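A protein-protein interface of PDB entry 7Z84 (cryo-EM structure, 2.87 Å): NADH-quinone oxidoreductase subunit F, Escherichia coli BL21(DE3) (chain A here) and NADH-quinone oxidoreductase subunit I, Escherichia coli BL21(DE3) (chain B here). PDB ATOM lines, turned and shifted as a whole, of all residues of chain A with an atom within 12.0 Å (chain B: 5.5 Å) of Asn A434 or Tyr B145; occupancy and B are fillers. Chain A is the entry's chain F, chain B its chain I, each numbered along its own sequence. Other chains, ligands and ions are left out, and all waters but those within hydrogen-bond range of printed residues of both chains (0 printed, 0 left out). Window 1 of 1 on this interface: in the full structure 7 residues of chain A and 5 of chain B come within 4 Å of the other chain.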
ATOM      1  N   THR A 430     -21.476  36.343  18.192  1.00  0.00           N
ATOM      2  CA  THR A 430     -21.935  34.995  18.474  1.00  0.00           C
ATOM      3  C   THR A 430     -20.960  33.981  17.900  1.00  0.00           C
ATOM      4  O   THR A 430     -20.308  34.226  16.882  1.00  0.00           O
ATOM      5  CB  THR A 430     -23.325  34.746  17.877  1.00  0.00           C
ATOM      6  OG1 THR A 430     -23.204  34.507  16.471  1.00  0.00           O
ATOM      7  CG2 THR A 430     -24.223  35.944  18.090  1.00  0.00           C
ATOM      8  N   HIS A 431     -20.863  32.840  18.567  1.00  0.00           N
ATOM      9  CA  HIS A 431     -20.168  31.684  18.028  1.00  0.00           C
ATOM     10  C   HIS A 431     -21.187  30.687  17.495  1.00  0.00           C
ATOM     11  O   HIS A 431     -22.361  30.704  17.872  1.00  0.00           O
ATOM     12  CB  HIS A 431     -19.284  31.033  19.092  1.00  0.00           C
ATOM     13  CG  HIS A 431     -20.017  30.669  20.342  1.00  0.00           C
ATOM     14  ND1 HIS A 431     -20.799  29.539  20.446  1.00  0.00           N
ATOM     15  CD2 HIS A 431     -20.095  31.292  21.541  1.00  0.00           C
ATOM     16  CE1 HIS A 431     -21.323  29.479  21.656  1.00  0.00           C
ATOM     17  NE2 HIS A 431     -20.913  30.532  22.340  1.00  0.00           N
ATOM     18  N   LEU A 432     -20.724  29.823  16.597  1.00  0.00           N
ATOM     19  CA  LEU A 432     -21.616  28.866  15.958  1.00  0.00           C
ATOM     20  C   LEU A 432     -22.075  27.804  16.950  1.00  0.00           C
ATOM     21  O   LEU A 432     -21.277  27.252  17.710  1.00  0.00           O
ATOM     22  CB  LEU A 432     -20.925  28.207  14.767  1.00  0.00           C
ATOM     23  CG  LEU A 432     -21.224  28.825  13.401  1.00  0.00           C
ATOM     24  CD1 LEU A 432     -20.122  29.787  12.989  1.00  0.00           C
ATOM     25  CD2 LEU A 432     -21.417  27.741  12.353  1.00  0.00           C
ATOM     26  N   ILE A 433     -23.374  27.529  16.938  1.00  0.00           N
ATOM     27  CA  ILE A 433     -23.969  26.457  17.726  1.00  0.00           C
ATOM     28  C   ILE A 433     -24.429  25.383  16.753  1.00  0.00           C
ATOM     29  O   ILE A 433     -25.217  25.660  15.841  1.00  0.00           O
ATOM     30  CB  ILE A 433     -25.132  26.961  18.592  1.00  0.00           C
ATOM     31  CG1 ILE A 433     -24.611  27.879  19.696  1.00  0.00           C
ATOM     32  CG2 ILE A 433     -25.891  25.795  19.199  1.00  0.00           C
ATOM     33  CD1 ILE A 433     -25.688  28.684  20.370  1.00  0.00           C
ATOM     34  N   ASN A 434     -23.923  24.166  16.935  1.00  0.00           N
ATOM     35  CA  ASN A 434     -24.232  23.076  16.020  1.00  0.00           C
ATOM     36  C   ASN A 434     -25.692  22.662  16.154  1.00  0.00           C
ATOM     37  O   ASN A 434     -26.226  22.573  17.263  1.00  0.00           O
ATOM     38  CB  ASN A 434     -23.315  21.886  16.290  1.00  0.00           C
ATOM     39  CG  ASN A 434     -23.136  21.002  15.076  1.00  0.00           C
ATOM     40  OD1 ASN A 434     -23.726  21.247  14.024  1.00  0.00           O
ATOM     41  ND2 ASN A 434     -22.316  19.968  15.213  1.00  0.00           N
ATOM     42  N   GLY A 435     -26.339  22.415  15.018  1.00  0.00           N
ATOM     43  CA  GLY A 435     -27.725  22.012  14.985  1.00  0.00           C
ATOM     44  C   GLY A 435     -28.718  23.150  14.895  1.00  0.00           C
ATOM     45  O   GLY A 435     -29.918  22.888  14.747  1.00  0.00           O
ATOM     46  N   ILE A 436     -28.262  24.395  14.982  1.00  0.00           N
ATOM     47  CA  ILE A 436     -29.126  25.567  14.888  1.00  0.00           C
ATOM     48  C   ILE A 436     -28.606  26.446  13.761  1.00  0.00           C
ATOM     49  O   ILE A 436     -27.459  26.907  13.805  1.00  0.00           O
ATOM     50  CB  ILE A 436     -29.177  26.349  16.209  1.00  0.00           C
ATOM     51  CG1 ILE A 436     -29.823  25.501  17.300  1.00  0.00           C
ATOM     52  CG2 ILE A 436     -29.939  27.650  16.028  1.00  0.00           C
ATOM     53  CD1 ILE A 436     -29.638  26.047  18.685  1.00  0.00           C
ATOM     54  N   GLN A 437     -29.445  26.680  12.762  1.00  0.00           N
ATOM     55  CA  GLN A 437     -29.083  27.581  11.676  1.00  0.00           C
ATOM     56  C   GLN A 437     -29.270  29.026  12.123  1.00  0.00           C
ATOM     57  O   GLN A 437     -30.353  29.386  12.593  1.00  0.00           O
ATOM     58  CB  GLN A 437     -29.922  27.296  10.436  1.00  0.00           C
ATOM     59  CG  GLN A 437     -29.464  26.076   9.660  1.00  0.00           C
ATOM     60  CD  GLN A 437     -30.537  25.527   8.743  1.00  0.00           C
ATOM     61  OE1 GLN A 437     -31.521  24.948   9.198  1.00  0.00           O
ATOM     62  NE2 GLN A 437     -30.349  25.702   7.441  1.00  0.00           N
ATOM     63  N   PRO A 438     -28.250  29.871  12.003  1.00  0.00           N
ATOM     64  CA  PRO A 438     -28.357  31.237  12.519  1.00  0.00           C
ATOM     65  C   PRO A 438     -29.223  32.120  11.633  1.00  0.00           C
ATOM     66  O   PRO A 438     -29.483  31.825  10.465  1.00  0.00           O
ATOM     67  CB  PRO A 438     -26.905  31.722  12.530  1.00  0.00           C
ATOM     68  CG  PRO A 438     -26.264  30.959  11.426  1.00  0.00           C
ATOM     69  CD  PRO A 438     -26.934  29.611  11.394  1.00  0.00           C
ATOM     70  N   ASN A 439     -29.678  33.223  12.223  1.00  0.00           N
ATOM     71  CA  ASN A 439     -30.464  34.226  11.509  1.00  0.00           C
ATOM     72  C   ASN A 439     -29.497  35.154  10.787  1.00  0.00           C
ATOM     73  O   ASN A 439     -28.867  36.018  11.401  1.00  0.00           O
ATOM     74  CB  ASN A 439     -31.357  34.993  12.476  1.00  0.00           C
ATOM     75  CG  ASN A 439     -32.591  35.557  11.805  1.00  0.00           C
ATOM     76  OD1 ASN A 439     -33.165  34.936  10.914  1.00  0.00           O
ATOM     77  ND2 ASN A 439     -33.006  36.744  12.233  1.00  0.00           N
ATOM     78  N   ARG B  59     -29.043  17.785  30.653  1.00  0.00           N
ATOM     79  CA  ARG B  59     -29.038  19.186  30.259  1.00  0.00           C
ATOM     80  C   ARG B  59     -30.171  19.992  30.876  1.00  0.00           C
ATOM     81  O   ARG B  59     -30.106  21.225  30.867  1.00  0.00           O
ATOM     82  CB  ARG B  59     -29.110  19.308  28.737  1.00  0.00           C
ATOM     83  CG  ARG B  59     -27.773  19.225  28.051  1.00  0.00           C
ATOM     84  CD  ARG B  59     -27.774  19.972  26.738  1.00  0.00           C
ATOM     85  NE  ARG B  59     -28.180  19.126  25.624  1.00  0.00           N
ATOM     86  CZ  ARG B  59     -27.509  19.016  24.488  1.00  0.00           C
ATOM     87  NH1 ARG B  59     -26.382  19.675  24.286  1.00  0.00           N
ATOM     88  NH2 ARG B  59     -27.980  18.223  23.531  1.00  0.00           N
ATOM     89  N   GLU B 106     -39.601  22.106  22.707  1.00  0.00           N
ATOM     90  CA  GLU B 106     -38.225  22.115  22.225  1.00  0.00           C
ATOM     91  C   GLU B 106     -37.815  23.508  21.774  1.00  0.00           C
ATOM     92  O   GLU B 106     -36.681  23.939  22.009  1.00  0.00           O
ATOM     93  CB  GLU B 106     -38.065  21.103  21.090  1.00  0.00           C
ATOM     94  CG  GLU B 106     -36.719  21.148  20.390  1.00  0.00           C
ATOM     95  CD  GLU B 106     -36.643  20.212  19.204  1.00  0.00           C
ATOM     96  OE1 GLU B 106     -37.532  19.348  19.064  1.00  0.00           O
ATOM     97  OE2 GLU B 106     -35.692  20.344  18.406  1.00  0.00           O
ATOM     98  N   THR B 112     -31.520  23.303  25.338  1.00  0.00           N
ATOM     99  CA  THR B 112     -31.640  22.229  24.338  1.00  0.00           C
ATOM    100  C   THR B 112     -31.682  20.851  24.993  1.00  0.00           C
ATOM    101  O   THR B 112     -31.116  19.881  24.487  1.00  0.00           O
ATOM    102  CB  THR B 112     -30.526  22.296  23.287  1.00  0.00           C
ATOM    103  OG1 THR B 112     -29.288  21.866  23.867  1.00  0.00           O
ATOM    104  CG2 THR B 112     -30.375  23.706  22.747  1.00  0.00           C
ATOM    105  N   GLN B 115     -36.111  17.463  23.452  1.00  0.00           N
ATOM    106  CA  GLN B 115     -35.997  17.368  22.005  1.00  0.00           C
ATOM    107  C   GLN B 115     -37.065  16.429  21.475  1.00  0.00           C
ATOM    108  O   GLN B 115     -37.521  15.524  22.173  1.00  0.00           O
ATOM    109  CB  GLN B 115     -34.613  16.869  21.566  1.00  0.00           C
ATOM    110  CG  GLN B 115     -33.487  17.865  21.764  1.00  0.00           C
ATOM    111  CD  GLN B 115     -32.125  17.244  21.567  1.00  0.00           C
ATOM    112  OE1 GLN B 115     -31.991  16.222  20.897  1.00  0.00           O
ATOM    113  NE2 GLN B 115     -31.108  17.845  22.164  1.00  0.00           N
ATOM    114  N   PRO B 142     -26.291  13.537  23.606  1.00  0.00           N
ATOM    115  CA  PRO B 142     -26.752  14.916  23.394  1.00  0.00           C
ATOM    116  C   PRO B 142     -27.921  15.062  22.435  1.00  0.00           C
ATOM    117  O   PRO B 142     -28.538  16.135  22.409  1.00  0.00           O
ATOM    118  CB  PRO B 142     -25.506  15.607  22.833  1.00  0.00           C
ATOM    119  CG  PRO B 142     -24.781  14.526  22.127  1.00  0.00           C
ATOM    120  CD  PRO B 142     -25.018  13.269  22.917  1.00  0.00           C
ATOM    121  N   GLY B 143     -28.249  14.040  21.653  1.00  0.00           N
ATOM    122  CA  GLY B 143     -29.341  14.160  20.709  1.00  0.00           C
ATOM    123  C   GLY B 143     -28.990  14.975  19.483  1.00  0.00           C
ATOM    124  O   GLY B 143     -27.942  14.760  18.867  1.00  0.00           O
ATOM    125  N   LYS B 144     -29.859  15.919  19.119  1.00  0.00           N
ATOM    126  CA  LYS B 144     -29.693  16.698  17.899  1.00  0.00           C
ATOM    127  C   LYS B 144     -28.728  17.867  18.048  1.00  0.00           C
ATOM    128  O   LYS B 144     -28.342  18.458  17.034  1.00  0.00           O
ATOM    129  CB  LYS B 144     -31.048  17.226  17.429  1.00  0.00           C
ATOM    130  CG  LYS B 144     -32.083  16.144  17.192  1.00  0.00           C
ATOM    131  CD  LYS B 144     -33.322  16.709  16.530  1.00  0.00           C
ATOM    132  CE  LYS B 144     -34.043  17.664  17.455  1.00  0.00           C
ATOM    133  NZ  LYS B 144     -35.329  18.120  16.869  1.00  0.00           N
ATOM    134  N   TYR B 145     -28.338  18.223  19.267  1.00  0.00           N
ATOM    135  CA  TYR B 145     -27.411  19.331  19.503  1.00  0.00           C
ATOM    136  C   TYR B 145     -26.193  18.791  20.237  1.00  0.00           C
ATOM    137  O   TYR B 145     -26.216  18.657  21.473  1.00  0.00           O
ATOM    138  CB  TYR B 145     -28.084  20.449  20.296  1.00  0.00           C
ATOM    139  CG  TYR B 145     -29.409  20.870  19.700  1.00  0.00           C
ATOM    140  CD1 TYR B 145     -29.462  21.752  18.630  1.00  0.00           C
ATOM    141  CD2 TYR B 145     -30.606  20.375  20.199  1.00  0.00           C
ATOM    142  CE1 TYR B 145     -30.670  22.129  18.077  1.00  0.00           C
ATOM    143  CE2 TYR B 145     -31.816  20.747  19.653  1.00  0.00           C
ATOM    144  CZ  TYR B 145     -31.843  21.627  18.593  1.00  0.00           C
ATOM    145  OH  TYR B 145     -33.048  22.002  18.047  1.00  0.00           O
ATOM    146  N   PRO B 146     -25.111  18.466  19.523  1.00  0.00           N
ATOM    147  CA  PRO B 146     -24.048  17.643  20.115  1.00  0.00           C
ATOM    148  C   PRO B 146     -23.089  18.371  21.042  1.00  0.00           C
ATOM    149  O   PRO B 146     -22.313  17.696  21.732  1.00  0.00           O
ATOM    150  CB  PRO B 146     -23.306  17.112  18.883  1.00  0.00           C
ATOM    151  CG  PRO B 146     -23.505  18.166  17.858  1.00  0.00           C
ATOM    152  CD  PRO B 146     -24.872  18.740  18.096  1.00  0.00           C
ATOM    153  N   GLU B 147     -23.095  19.703  21.095  1.00  0.00           N
ATOM    154  CA  GLU B 147     -22.063  20.409  21.843  1.00  0.00           C
ATOM    155  C   GLU B 147     -22.561  21.517  22.759  1.00  0.00           C
ATOM    156  O   GLU B 147     -21.751  22.048  23.526  1.00  0.00           O
ATOM    157  CB  GLU B 147     -21.016  20.995  20.882  1.00  0.00           C
ATOM    158  CG  GLU B 147     -21.589  21.663  19.637  1.00  0.00           C
ATOM    159  CD  GLU B 147     -21.900  23.139  19.828  1.00  0.00           C
ATOM    160  OE1 GLU B 147     -22.457  23.748  18.894  1.00  0.00           O
ATOM    161  OE2 GLU B 147     -21.562  23.701  20.890  1.00  0.00           O
ATOM    162  N   TYR B 148     -23.837  21.889  22.711  1.00  0.00           N
ATOM    163  CA  TYR B 148     -24.299  23.010  23.521  1.00  0.00           C
ATOM    164  C   TYR B 148     -24.387  22.618  24.991  1.00  0.00           C
ATOM    165  O   TYR B 148     -24.946  21.573  25.337  1.00  0.00           O
ATOM    166  CB  TYR B 148     -25.658  23.513  23.042  1.00  0.00           C
ATOM    167  CG  TYR B 148     -26.111  24.733  23.810  1.00  0.00           C
ATOM    168  CD1 TYR B 148     -25.458  25.947  23.662  1.00  0.00           C
ATOM    169  CD2 TYR B 148     -27.165  24.661  24.710  1.00  0.00           C
ATOM    170  CE1 TYR B 148     -25.854  27.061  24.371  1.00  0.00           C
ATOM    171  CE2 TYR B 148     -27.566  25.772  25.426  1.00  0.00           C
ATOM    172  CZ  TYR B 148     -26.908  26.968  25.251  1.00  0.00           C
ATOM    173  OH  TYR B 148     -27.303  28.078  25.958  1.00  0.00           O
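The backbone NH of Asn A434 lies within hydrogen-bond range of the side-chain carboxylate of Glu B147, 2.5 Å away.
The side-chain carboxylate (OE2) of Glu B106 is in hydrogen-bond range of the side-chain hydroxyl (OH) of Tyr B145 (3.1 Å).
NH2 of Arg B59 sits at hydrogen-bond distance from O of Tyr B145 (2.7 Å).
Among the printed residues, merely in contact across the chains: Ile A433 with Glu B147 (3.3 Å), Asn A434 with Pro B146 (3.4 Å), Gly A435 with Tyr B145 (3.5 Å), Ile A436 with Tyr B145 (3.6 Å), Asn A434 with Tyr B145 (3.6 Å) and Leu A432 with Glu B147 (3.9 Å).
His A431 touches none of the printed residues of chain B.
Printed residues of chain B within 4 Å of Leu A432: Glu B147 (3.9 Å).
Printed residues of chain B within 4 Å of Ile A433: Glu B147 (3.3 Å).
Of chain B, only Tyr B145, Pro B146 and Glu B147 come within 4 Å of Asn A434.
Printed residues of chain B within 4 Å of Gly A435: Tyr B145 (3.5 Å).
Of the printed residues of chain B, Ile A436 touches Tyr B145 (3.6 Å).
Gln A437 touches none of the printed residues of chain B.
No residue of chain A comes within 4 Å of Pro B142.
No residue of chain A comes within 4 Å of Gly B143.
Tyr B145 touches just these residues of chain A: Asn A434, Gly A435 and Ile A436.
Of chain A, only Asn A434 comes within 4 Å of Pro B146.
Printed residues of chain A within 4 Å of Glu B147: Leu A432, Ile A433 and Asn A434.
The nearest printed residue of chain B that does not touch Ile A436 is Thr B112 (4.7 Å).
Printed residues of chain A that touch a printed residue of chain B: Leu A432, Ile A433, Asn A434, Gly A435 and Ile A436.
Printed residues of chain B that touch a printed residue of chain A: Tyr B145, Pro B146 and Glu B147.
Hydrophobic or aromatic side chains of chain B that line the printed part of chain A: Tyr B145 and Pro B146.
Among the printed residues, 7 pairs touch across the chains.
Among the printed residues, no Asp or Glu carboxylate lies within 4 Å of a Lys or Arg side-chain nitrogen of the other chain.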
